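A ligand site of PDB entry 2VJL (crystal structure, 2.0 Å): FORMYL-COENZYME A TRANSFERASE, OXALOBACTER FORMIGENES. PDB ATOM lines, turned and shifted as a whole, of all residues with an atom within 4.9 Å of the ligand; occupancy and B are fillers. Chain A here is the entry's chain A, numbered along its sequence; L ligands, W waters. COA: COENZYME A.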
ATOM      1  N   HIS A  15      25.888  33.336 -32.022  1.00  0.00           N
ATOM      2  CA  HIS A  15      26.184  34.513 -31.226  1.00  0.00           C
ATOM      3  C   HIS A  15      27.497  35.158 -31.697  1.00  0.00           C
ATOM      4  O   HIS A  15      28.237  34.568 -32.493  1.00  0.00           O
ATOM      5  CB  HIS A  15      26.251  34.148 -29.744  1.00  0.00           C
ATOM      6  CG  HIS A  15      27.398  33.244 -29.398  1.00  0.00           C
ATOM      7  ND1 HIS A  15      28.230  33.481 -28.328  1.00  0.00           N
ATOM      8  CD2 HIS A  15      27.859  32.103 -29.974  1.00  0.00           C
ATOM      9  CE1 HIS A  15      29.141  32.535 -28.258  1.00  0.00           C
ATOM     10  NE2 HIS A  15      28.944  31.680 -29.245  1.00  0.00           N
ATOM     11  N   VAL A  16      27.772  36.346 -31.189  1.00  0.00           N
ATOM     12  CA  VAL A  16      28.969  37.129 -31.532  1.00  0.00           C
ATOM     13  C   VAL A  16      29.073  37.468 -33.046  1.00  0.00           C
ATOM     14  O   VAL A  16      28.196  38.160 -33.556  1.00  0.00           O
ATOM     15  CB  VAL A  16      30.277  36.577 -30.859  1.00  0.00           C
ATOM     16  CG1 VAL A  16      30.138  36.669 -29.349  1.00  0.00           C
ATOM     17  CG2 VAL A  16      30.567  35.134 -31.245  1.00  0.00           C
ATOM     18  N   GLN A  17      30.094  36.993 -33.773  1.00  0.00           N
ATOM     19  CA  GLN A  17      30.324  37.515 -35.142  1.00  0.00           C
ATOM     20  C   GLN A  17      30.144  36.519 -36.297  1.00  0.00           C
ATOM     21  O   GLN A  17      29.364  36.788 -37.223  1.00  0.00           O
ATOM     22  CB  GLN A  17      31.718  38.139 -35.214  1.00  0.00           C
ATOM     23  CG  GLN A  17      31.831  39.435 -34.454  1.00  0.00           C
ATOM     24  CD  GLN A  17      33.255  39.930 -34.367  1.00  0.00           C
ATOM     25  OE1 GLN A  17      33.822  40.424 -35.343  1.00  0.00           O
ATOM     26  NE2 GLN A  17      33.857  39.817 -33.185  1.00  0.00           N
ATOM     27  N   ALA A  18      30.853  35.391 -36.258  1.00  0.00           N
ATOM     28  CA  ALA A  18      30.889  34.452 -37.394  1.00  0.00           C
ATOM     29  C   ALA A  18      29.527  33.878 -37.763  1.00  0.00           C
ATOM     30  O   ALA A  18      29.091  33.961 -38.915  1.00  0.00           O
ATOM     31  CB  ALA A  18      31.859  33.318 -37.112  1.00  0.00           C
ATOM     32  N   ILE A  36      17.591  32.066 -31.563  1.00  0.00           N
ATOM     33  CA  ILE A  36      17.454  31.562 -30.199  1.00  0.00           C
ATOM     34  C   ILE A  36      18.512  32.214 -29.307  1.00  0.00           C
ATOM     35  O   ILE A  36      19.714  32.063 -29.555  1.00  0.00           O
ATOM     36  CB  ILE A  36      17.611  30.030 -30.121  1.00  0.00           C
ATOM     37  CG1 ILE A  36      16.450  29.347 -30.844  1.00  0.00           C
ATOM     38  CG2 ILE A  36      17.678  29.566 -28.678  1.00  0.00           C
ATOM     39  CD1 ILE A  36      16.496  27.855 -30.769  1.00  0.00           C
ATOM     40  N   GLU A  37      18.048  32.917 -28.268  1.00  0.00           N
ATOM     41  CA  GLU A  37      18.939  33.607 -27.333  1.00  0.00           C
ATOM     42  C   GLU A  37      18.609  33.200 -25.904  1.00  0.00           C
ATOM     43  O   GLU A  37      17.489  32.780 -25.613  1.00  0.00           O
ATOM     44  CB  GLU A  37      18.786  35.121 -27.482  1.00  0.00           C
ATOM     45  CG  GLU A  37      18.912  35.614 -28.911  1.00  0.00           C
ATOM     46  CD  GLU A  37      18.993  37.132 -29.003  1.00  0.00           C
ATOM     47  OE1 GLU A  37      19.958  37.711 -28.469  1.00  0.00           O
ATOM     48  OE2 GLU A  37      18.092  37.729 -29.621  1.00  0.00           O
ATOM     49  N   ARG A  38      19.583  33.321 -25.007  1.00  0.00           N
ATOM     50  CA  ARG A  38      19.346  33.067 -23.587  1.00  0.00           C
ATOM     51  C   ARG A  38      18.613  34.250 -22.946  1.00  0.00           C
ATOM     52  O   ARG A  38      18.728  35.386 -23.400  1.00  0.00           O
ATOM     53  CB  ARG A  38      20.632  32.721 -22.813  1.00  0.00           C
ATOM     54  CG  ARG A  38      21.886  33.510 -23.171  1.00  0.00           C
ATOM     55  CD  ARG A  38      22.868  33.541 -21.998  1.00  0.00           C
ATOM     56  NE  ARG A  38      24.254  33.251 -22.385  1.00  0.00           N
ATOM     57  CZ  ARG A  38      24.880  32.081 -22.234  1.00  0.00           C
ATOM     58  NH1 ARG A  38      26.136  31.951 -22.622  1.00  0.00           N
ATOM     59  NH2 ARG A  38      24.258  31.022 -21.702  1.00  0.00           N
ATOM     60  N   LEU A  72      15.120  31.633 -24.745  1.00  0.00           N
ATOM     61  CA  LEU A  72      14.976  30.208 -24.425  1.00  0.00           C
ATOM     62  C   LEU A  72      16.113  29.672 -23.552  1.00  0.00           C
ATOM     63  O   LEU A  72      17.273  29.701 -23.943  1.00  0.00           O
ATOM     64  CB  LEU A  72      14.863  29.384 -25.712  1.00  0.00           C
ATOM     65  CG  LEU A  72      14.617  27.873 -25.586  1.00  0.00           C
ATOM     66  CD1 LEU A  72      13.452  27.571 -24.655  1.00  0.00           C
ATOM     67  CD2 LEU A  72      14.382  27.253 -26.957  1.00  0.00           C
ATOM     68  N   ASP A  73      15.750  29.204 -22.360  1.00  0.00           N
ATOM     69  CA  ASP A  73      16.656  28.400 -21.545  1.00  0.00           C
ATOM     70  C   ASP A  73      16.602  26.970 -22.085  1.00  0.00           C
ATOM     71  O   ASP A  73      15.583  26.288 -21.953  1.00  0.00           O
ATOM     72  CB  ASP A  73      16.244  28.448 -20.062  1.00  0.00           C
ATOM     73  CG  ASP A  73      17.319  27.920 -19.134  1.00  0.00           C
ATOM     74  OD1 ASP A  73      17.878  26.837 -19.392  1.00  0.00           O
ATOM     75  OD2 ASP A  73      17.602  28.595 -18.115  1.00  0.00           O
ATOM     76  N   MET A  74      17.692  26.538 -22.720  1.00  0.00           N
ATOM     77  CA  MET A  74      17.759  25.236 -23.375  1.00  0.00           C
ATOM     78  C   MET A  74      18.236  24.117 -22.446  1.00  0.00           C
ATOM     79  O   MET A  74      18.154  22.934 -22.794  1.00  0.00           O
ATOM     80  CB  MET A  74      18.654  25.302 -24.616  1.00  0.00           C
ATOM     81  CG  MET A  74      18.125  26.227 -25.710  1.00  0.00           C
ATOM     82  SD  MET A  74      19.187  26.305 -27.174  1.00  0.00           S
ATOM     83  CE  MET A  74      20.671  27.030 -26.483  1.00  0.00           C
ATOM     84  N   LYS A  75      18.716  24.483 -21.254  1.00  0.00           N
ATOM     85  CA  LYS A  75      19.071  23.509 -20.220  1.00  0.00           C
ATOM     86  C   LYS A  75      17.891  23.322 -19.256  1.00  0.00           C
ATOM     87  O   LYS A  75      18.047  23.394 -18.035  1.00  0.00           O
ATOM     88  CB  LYS A  75      20.337  23.954 -19.468  1.00  0.00           C
ATOM     89  CG  LYS A  75      21.604  23.926 -20.326  1.00  0.00           C
ATOM     90  CD  LYS A  75      22.808  24.489 -19.576  1.00  0.00           C
ATOM     91  CE  LYS A  75      24.092  24.346 -20.394  1.00  0.00           C
ATOM     92  NZ  LYS A  75      25.265  24.983 -19.738  1.00  0.00           N
ATOM     93  N   ASN A  96      27.446  28.470 -33.504  1.00  0.00           N
ATOM     94  CA  ASN A  96      28.870  28.660 -33.239  1.00  0.00           C
ATOM     95  C   ASN A  96      29.117  28.774 -31.732  1.00  0.00           C
ATOM     96  O   ASN A  96      29.678  29.751 -31.247  1.00  0.00           O
ATOM     97  CB  ASN A  96      29.455  29.855 -34.037  1.00  0.00           C
ATOM     98  CG  ASN A  96      28.948  31.212 -33.555  1.00  0.00           C
ATOM     99  OD1 ASN A  96      27.797  31.353 -33.167  1.00  0.00           O
ATOM    100  ND2 ASN A  96      29.824  32.219 -33.604  1.00  0.00           N
ATOM    101  N   PHE A  97      28.672  27.749 -31.014  1.00  0.00           N
ATOM    102  CA  PHE A  97      29.053  27.554 -29.613  1.00  0.00           C
ATOM    103  C   PHE A  97      30.464  26.952 -29.595  1.00  0.00           C
ATOM    104  O   PHE A  97      31.057  26.727 -30.655  1.00  0.00           O
ATOM    105  CB  PHE A  97      28.100  26.597 -28.879  1.00  0.00           C
ATOM    106  CG  PHE A  97      26.711  27.152 -28.648  1.00  0.00           C
ATOM    107  CD1 PHE A  97      25.591  26.386 -28.950  1.00  0.00           C
ATOM    108  CD2 PHE A  97      26.536  28.427 -28.118  1.00  0.00           C
ATOM    109  CE1 PHE A  97      24.316  26.878 -28.736  1.00  0.00           C
ATOM    110  CE2 PHE A  97      25.246  28.926 -27.898  1.00  0.00           C
ATOM    111  CZ  PHE A  97      24.143  28.143 -28.205  1.00  0.00           C
ATOM    112  N   GLY A  98      30.982  26.688 -28.402  1.00  0.00           N
ATOM    113  CA  GLY A  98      32.185  25.882 -28.252  1.00  0.00           C
ATOM    114  C   GLY A  98      31.966  24.460 -28.756  1.00  0.00           C
ATOM    115  O   GLY A  98      30.825  24.016 -28.867  1.00  0.00           O
ATOM    116  N   PRO A  99      33.063  23.742 -29.077  1.00  0.00           N
ATOM    117  CA  PRO A  99      33.043  22.408 -29.694  1.00  0.00           C
ATOM    118  C   PRO A  99      31.984  21.403 -29.188  1.00  0.00           C
ATOM    119  O   PRO A  99      31.181  20.923 -29.990  1.00  0.00           O
ATOM    120  CB  PRO A  99      34.458  21.894 -29.408  1.00  0.00           C
ATOM    121  CG  PRO A  99      35.292  23.110 -29.445  1.00  0.00           C
ATOM    122  CD  PRO A  99      34.442  24.226 -28.888  1.00  0.00           C
ATOM    123  N   ALA A 101      29.421  21.828 -27.034  1.00  0.00           N
ATOM    124  CA  ALA A 101      28.238  22.469 -26.433  1.00  0.00           C
ATOM    125  C   ALA A 101      26.883  21.890 -26.862  1.00  0.00           C
ATOM    126  O   ALA A 101      26.030  21.609 -26.018  1.00  0.00           O
ATOM    127  CB  ALA A 101      28.261  23.971 -26.687  1.00  0.00           C
ATOM    128  N   ARG A 104      26.273  18.036 -25.813  1.00  0.00           N
ATOM    129  CA  ARG A 104      26.029  17.878 -24.367  1.00  0.00           C
ATOM    130  C   ARG A 104      24.657  18.391 -23.911  1.00  0.00           C
ATOM    131  O   ARG A 104      24.284  18.233 -22.743  1.00  0.00           O
ATOM    132  CB  ARG A 104      27.149  18.548 -23.562  1.00  0.00           C
ATOM    133  CG  ARG A 104      28.413  17.692 -23.454  1.00  0.00           C
ATOM    134  CD  ARG A 104      29.453  18.292 -22.513  1.00  0.00           C
ATOM    135  NE  ARG A 104      30.473  19.048 -23.241  1.00  0.00           N
ATOM    136  CZ  ARG A 104      30.389  20.340 -23.561  1.00  0.00           C
ATOM    137  NH1 ARG A 104      29.319  21.066 -23.232  1.00  0.00           N
ATOM    138  NH2 ARG A 104      31.386  20.918 -24.227  1.00  0.00           N
ATOM    139  N   MET A 105      23.900  18.996 -24.821  1.00  0.00           N
ATOM    140  CA  MET A 105      22.490  19.324 -24.589  1.00  0.00           C
ATOM    141  C   MET A 105      21.554  18.187 -25.022  1.00  0.00           C
ATOM    142  O   MET A 105      20.336  18.323 -24.935  1.00  0.00           O
ATOM    143  CB  MET A 105      22.110  20.611 -25.329  1.00  0.00           C
ATOM    144  CG  MET A 105      22.720  21.869 -24.735  1.00  0.00           C
ATOM    145  SD  MET A 105      21.969  23.331 -25.453  1.00  0.00           S
ATOM    146  CE  MET A 105      22.497  24.591 -24.300  1.00  0.00           C
ATOM    147  N   VAL A 124      30.332  26.701 -37.018  1.00  0.00           N
ATOM    148  CA  VAL A 124      31.638  27.348 -37.116  1.00  0.00           C
ATOM    149  C   VAL A 124      32.424  26.961 -35.872  1.00  0.00           C
ATOM    150  O   VAL A 124      31.887  27.032 -34.749  1.00  0.00           O
ATOM    151  CB  VAL A 124      31.557  28.904 -37.183  1.00  0.00           C
ATOM    152  CG1 VAL A 124      32.965  29.525 -37.147  1.00  0.00           C
ATOM    153  CG2 VAL A 124      30.809  29.344 -38.429  1.00  0.00           C
ATOM    154  N   LYS A 125      33.677  26.549 -36.064  1.00  0.00           N
ATOM    155  CA  LYS A 125      34.588  26.158 -34.991  1.00  0.00           C
ATOM    156  C   LYS A 125      35.914  26.884 -35.180  1.00  0.00           C
ATOM    157  O   LYS A 125      36.193  27.404 -36.252  1.00  0.00           O
ATOM    158  CB  LYS A 125      34.842  24.649 -35.052  1.00  0.00           C
ATOM    159  CG  LYS A 125      33.626  23.785 -35.399  1.00  0.00           C
ATOM    160  CD  LYS A 125      34.037  22.369 -35.782  1.00  0.00           C
ATOM    161  CE  LYS A 125      32.829  21.489 -36.022  1.00  0.00           C
ATOM    162  NZ  LYS A 125      33.209  20.081 -36.342  1.00  0.00           N
ATOM    163  N   GLY A 126      36.745  26.895 -34.144  1.00  0.00           N
ATOM    164  CA  GLY A 126      38.085  27.446 -34.250  1.00  0.00           C
ATOM    165  C   GLY A 126      38.972  26.577 -35.118  1.00  0.00           C
ATOM    166  O   GLY A 126      39.628  27.083 -36.038  1.00  0.00           O
ATOM    167  N   LEU A 136      39.527  23.720 -28.767  1.00  0.00           N
ATOM    168  CA  LEU A 136      39.822  25.086 -28.311  1.00  0.00           C
ATOM    169  C   LEU A 136      38.748  26.101 -28.703  1.00  0.00           C
ATOM    170  O   LEU A 136      38.142  26.015 -29.784  1.00  0.00           O
ATOM    171  CB  LEU A 136      41.176  25.545 -28.858  1.00  0.00           C
ATOM    172  CG  LEU A 136      42.421  24.779 -28.404  1.00  0.00           C
ATOM    173  CD1 LEU A 136      43.663  25.368 -29.062  1.00  0.00           C
ATOM    174  CD2 LEU A 136      42.565  24.799 -26.882  1.00  0.00           C
ATOM    175  N   LYS A 137      38.521  27.068 -27.812  1.00  0.00           N
ATOM    176  CA  LYS A 137      37.720  28.262 -28.109  1.00  0.00           C
ATOM    177  C   LYS A 137      38.624  29.333 -28.726  1.00  0.00           C
ATOM    178  O   LYS A 137      39.682  29.649 -28.166  1.00  0.00           O
ATOM    179  CB  LYS A 137      37.077  28.813 -26.836  1.00  0.00           C
ATOM    180  CG  LYS A 137      36.013  27.902 -26.230  1.00  0.00           C
ATOM    181  CD  LYS A 137      35.428  28.504 -24.952  1.00  0.00           C
ATOM    182  CE  LYS A 137      34.425  27.565 -24.296  1.00  0.00           C
ATOM    183  NZ  LYS A 137      33.870  28.121 -23.029  1.00  0.00           N
ATOM    184  N   VAL A 138      38.226  29.881 -29.872  1.00  0.00           N
ATOM    185  CA  VAL A 138      39.077  30.804 -30.625  1.00  0.00           C
ATOM    186  C   VAL A 138      38.350  32.113 -30.935  1.00  0.00           C
ATOM    187  O   VAL A 138      37.184  32.101 -31.318  1.00  0.00           O
ATOM    188  CB  VAL A 138      39.545  30.162 -31.946  1.00  0.00           C
ATOM    189  CG1 VAL A 138      40.425  31.121 -32.732  1.00  0.00           C
ATOM    190  CG2 VAL A 138      40.292  28.854 -31.671  1.00  0.00           C
ATOM    191  N   TYR A 139      39.060  33.233 -30.766  1.00  0.00           N
ATOM    192  CA  TYR A 139      38.547  34.559 -31.118  1.00  0.00           C
ATOM    193  C   TYR A 139      39.248  35.112 -32.371  1.00  0.00           C
ATOM    194  O   TYR A 139      40.234  34.545 -32.824  1.00  0.00           O
ATOM    195  CB  TYR A 139      38.733  35.519 -29.940  1.00  0.00           C
ATOM    196  CG  TYR A 139      37.971  35.116 -28.689  1.00  0.00           C
ATOM    197  CD1 TYR A 139      36.616  35.417 -28.544  1.00  0.00           C
ATOM    198  CD2 TYR A 139      38.611  34.428 -27.654  1.00  0.00           C
ATOM    199  CE1 TYR A 139      35.913  35.043 -27.382  1.00  0.00           C
ATOM    200  CE2 TYR A 139      37.923  34.055 -26.509  1.00  0.00           C
ATOM    201  CZ  TYR A 139      36.577  34.369 -26.372  1.00  0.00           C
ATOM    202  OH  TYR A 139      35.904  33.990 -25.232  1.00  0.00           O
ATOM    203  N   GLU A 140      38.740  36.218 -32.902  1.00  0.00           N
ATOM    204  CA  GLU A 140      39.188  36.796 -34.178  1.00  0.00           C
ATOM    205  C   GLU A 140      40.708  36.733 -34.418  1.00  0.00           C
ATOM    206  O   GLU A 140      41.160  36.099 -35.379  1.00  0.00           O
ATOM    207  CB  GLU A 140      38.724  38.262 -34.291  1.00  0.00           C
ATOM    208  CG  GLU A 140      39.248  39.027 -35.519  1.00  0.00           C
ATOM    209  CD  GLU A 140      38.827  38.409 -36.852  1.00  0.00           C
ATOM    210  OE1 GLU A 140      39.702  38.238 -37.736  1.00  0.00           O
ATOM    211  OE2 GLU A 140      37.639  38.091 -37.022  1.00  0.00           O
ATOM    212  N   ASP A 169      36.399  35.837 -38.256  1.00  0.00           N
ATOM    213  CA  ASP A 169      34.969  35.722 -37.889  1.00  0.00           C
ATOM    214  C   ASP A 169      34.059  35.834 -39.098  1.00  0.00           C
ATOM    215  O   ASP A 169      33.487  34.831 -39.512  1.00  0.00           O
ATOM    216  CB  ASP A 169      34.614  36.757 -36.820  1.00  0.00           C
ATOM    217  CG  ASP A 169      34.957  36.264 -35.430  1.00  0.00           C
ATOM    218  OD1 ASP A 169      35.795  36.843 -34.756  1.00  0.00           O
ATOM    219  N   MET A 200      37.616  28.213 -38.397  1.00  0.00           N
ATOM    220  CA  MET A 200      38.153  29.558 -38.620  1.00  0.00           C
ATOM    221  C   MET A 200      39.586  29.497 -39.136  1.00  0.00           C
ATOM    222  O   MET A 200      39.945  30.275 -40.028  1.00  0.00           O
ATOM    223  CB  MET A 200      38.091  30.391 -37.343  1.00  0.00           C
ATOM    224  CG  MET A 200      36.671  30.676 -36.830  1.00  0.00           C
ATOM    225  SD  MET A 200      36.698  31.283 -35.133  1.00  0.00           S
ATOM    226  CE  MET A 200      37.116  32.992 -35.446  1.00  0.00           C
HETATM  227  N1A COA L   1      20.425  28.185 -22.998  1.00  0.00           N
HETATM  228  C2A COA L   1      21.192  27.336 -22.296  1.00  0.00           C
HETATM  229  N3A COA L   1      22.523  27.287 -22.467  1.00  0.00           N
HETATM  230  C4A COA L   1      23.128  28.118 -23.361  1.00  0.00           C
HETATM  231  C5A COA L   1      22.358  29.004 -24.097  1.00  0.00           C
HETATM  232  C6A COA L   1      20.982  29.032 -23.896  1.00  0.00           C
HETATM  233  N6A COA L   1      20.218  29.871 -24.598  1.00  0.00           N
HETATM  234  N7A COA L   1      23.201  29.697 -24.896  1.00  0.00           N
HETATM  235  C8A COA L   1      24.456  29.244 -24.658  1.00  0.00           C
HETATM  236  N9A COA L   1      24.408  28.282 -23.721  1.00  0.00           N
HETATM  237  C1B COA L   1      25.547  27.518 -23.163  1.00  0.00           C
HETATM  238  C2B COA L   1      26.253  26.647 -24.198  1.00  0.00           C
HETATM  239  O2B COA L   1      25.530  25.444 -24.494  1.00  0.00           O
HETATM  240  C3B COA L   1      27.581  26.377 -23.508  1.00  0.00           C
HETATM  241  O3B COA L   1      27.440  25.164 -22.756  1.00  0.00           O
HETATM  242  P3B COA L   1      28.674  24.366 -22.107  1.00  0.00           P
HETATM  243  O7A COA L   1      29.753  24.352 -23.166  1.00  0.00           O
HETATM  244  O8A COA L   1      29.023  25.064 -20.809  1.00  0.00           O
HETATM  245  O9A COA L   1      28.108  23.024 -21.705  1.00  0.00           O
HETATM  246  C4B COA L   1      27.789  27.584 -22.592  1.00  0.00           C
HETATM  247  O4B COA L   1      26.585  28.358 -22.659  1.00  0.00           O
HETATM  248  C5B COA L   1      29.001  28.429 -22.985  1.00  0.00           C
HETATM  249  O5B COA L   1      28.822  29.027 -24.268  1.00  0.00           O
HETATM  250  P1A COA L   1      29.967  28.908 -25.399  1.00  0.00           P
HETATM  251  O1A COA L   1      29.669  29.857 -26.530  1.00  0.00           O
HETATM  252  O2A COA L   1      30.068  27.486 -25.914  1.00  0.00           O
HETATM  253  O3A COA L   1      31.335  29.332 -24.637  1.00  0.00           O
HETATM  254  P2A COA L   1      31.793  30.875 -24.431  1.00  0.00           P
HETATM  255  O4A COA L   1      32.560  30.921 -23.134  1.00  0.00           O
HETATM  256  O5A COA L   1      30.611  31.801 -24.601  1.00  0.00           O
HETATM  257  O6A COA L   1      32.876  31.088 -25.622  1.00  0.00           O
HETATM  258  CBP COA L   1      33.334  31.513 -27.995  1.00  0.00           C
HETATM  259  CCP COA L   1      32.713  32.034 -26.683  1.00  0.00           C
HETATM  260  CDP COA L   1      33.002  32.507 -29.096  1.00  0.00           C
HETATM  261  CEP COA L   1      34.846  31.469 -27.801  1.00  0.00           C
HETATM  262  CAP COA L   1      32.776  30.123 -28.340  1.00  0.00           C
HETATM  263  OAP COA L   1      31.345  30.190 -28.459  1.00  0.00           O
HETATM  264  C9P COA L   1      33.340  29.547 -29.614  1.00  0.00           C
HETATM  265  O9P COA L   1      34.487  28.868 -29.578  1.00  0.00           O
HETATM  266  N8P COA L   1      32.661  29.717 -30.747  1.00  0.00           N
HETATM  267  C7P COA L   1      33.084  29.191 -32.043  1.00  0.00           C
HETATM  268  C6P COA L   1      34.100  30.074 -32.756  1.00  0.00           C
HETATM  269  C5P COA L   1      33.594  31.480 -32.995  1.00  0.00           C
HETATM  270  O5P COA L   1      32.506  31.671 -33.550  1.00  0.00           O
HETATM  271  N4P COA L   1      34.416  32.463 -32.590  1.00  0.00           N
HETATM  272  C3P COA L   1      33.969  33.794 -32.214  1.00  0.00           C
HETATM  273  C2P COA L   1      34.636  34.868 -33.078  1.00  0.00           C
HETATM  274  S1P COA L   1      34.025  34.848 -34.726  1.00  0.00           S
HETATM  275  O   HOH W   1      36.304  37.462 -31.678  1.00  0.00           O
HETATM  276  O   HOH W   2      25.614  22.809 -23.377  1.00  0.00           O
HETATM  277  O   HOH W   3      36.292  27.350 -31.217  1.00  0.00           O
HETATM  278  O   HOH W   4      27.403  31.724 -25.184  1.00  0.00           O
HETATM  279  O   HOH W   5      20.674  27.554 -19.087  1.00  0.00           O
HETATM  280  O   HOH W   6      34.983  30.791 -22.545  1.00  0.00           O
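CG of Asp 169 is covalently linked to S1P of the ligand (1.8 Å).
A nitrogen (N8P) of the ligand lies within hydrogen-bond range of the backbone carbonyl oxygen of Asn 96, at 3.0 Å.
ND2 of Asn 96 is in hydrogen-bond range of O5P of the ligand.
The guanidinium group (NH1) of Arg 104 is in salt-bridge range of an oxygen (O9A) of the ligand.
N of Gly 98 sits at hydrogen-bond distance from O2A of the ligand, 2.8 Å away.
A ring nitrogen (NE2) of His 15 sits at hydrogen-bond distance from an oxygen (OAP) of the ligand, at 2.9 Å.
The backbone carbonyl oxygen of Leu 72 is in hydrogen-bond range of a nitrogen (N6A) of the ligand, at 3.0 Å.
A nitrogen (N4P) of the ligand sits at hydrogen-bond distance from the backbone carbonyl oxygen (O) of Val 138 (3.1 Å).
O4A of the ligand lies within salt-bridge range of NZ of Lys 137.
N of Met 74 sits at hydrogen-bond distance from N1A of the ligand (3.2 Å).
A nitrogen (N8P) of the ligand sits at hydrogen-bond distance from the backbone carbonyl oxygen of Phe 97, at 3.4 Å.
The backbone NH (N) of Ala 18 sits close to a sulfur (S1P) of the ligand, at 3.6 Å.
N4P of the ligand is in hydrogen-bond range of SD of Met 200, at 3.6 Å.
The side-chain amino group (NZ) of Lys 75 lies within salt-bridge range of an oxygen (O8A) of the ligand (3.9 Å).
N of Asp 169 sits at hydrogen-bond distance from OE2 of Glu 140 (2.9 Å).
A ring nitrogen (NE2) of His 15 sits at hydrogen-bond distance from the backbone carbonyl oxygen of Asn 96 (2.9 Å).
The backbone carbonyl oxygen (O) of Glu 37 lies within hydrogen-bond range of the backbone NH (N) of Leu 72, at 2.8 Å.
The backbone NH (N) of Met 200 lies within hydrogen-bond range of the backbone carbonyl oxygen (O) of Gly 126 (3.3 Å).
The backbone carbonyl oxygen of Lys 125 is in hydrogen-bond range of the backbone NH of Met 200.
The backbone NH of Lys 75 sits at hydrogen-bond distance from the side-chain carboxylate of Asp 73 (3.1 Å).
NH2 of Arg 38 lies close to N9A of the ligand (3.4 Å).
Val 16 touches the ligand.
Glu 37 touches the ligand.
Ala 101 touches the ligand.
CE of Met 105 touches O2B of the ligand, 3.2 Å away.
O of Val 124 touches C7P of the ligand (3.7 Å).
CZ of Tyr 139 touches CEP of the ligand, 3.7 Å away.
Hydrophobic or aromatic side chains within 4 Å of the ligand: His 15, Val 16, Ala 18, Met 74, Phe 97, Ala 101, Met 105, Tyr 139 and Met 200.
Of the 28 residues printed, 20 come within 4 Å of the ligand.
The nearest printed residue that does not touch the ligand is Asp 73 (4.05 Å).
Water W6 lies within hydrogen-bond range of an oxygen (O4A) of the ligand (2.5 Å) and the side-chain amino group (NZ) of Lys 137 (2.9 Å).
Water W2 lies within hydrogen-bond range of O2B of the ligand (2.9 Å) and O of Ala 101 (2.9 Å).
Water W3 lies within hydrogen-bond range of O of Leu 136, O9P of the ligand, N of Gly 126 and N of Val 138.
Water W4 bridges the guanidinium group (NH1) of Arg 38 (2.9 Å) and an oxygen (O5B) of the ligand (3.2 Å).
Water W1 lies within hydrogen-bond range of the backbone NH (N) of Glu 140 (3.0 Å) and the side-chain carboxylate (OD1) of Asp 169 (3.2 Å).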
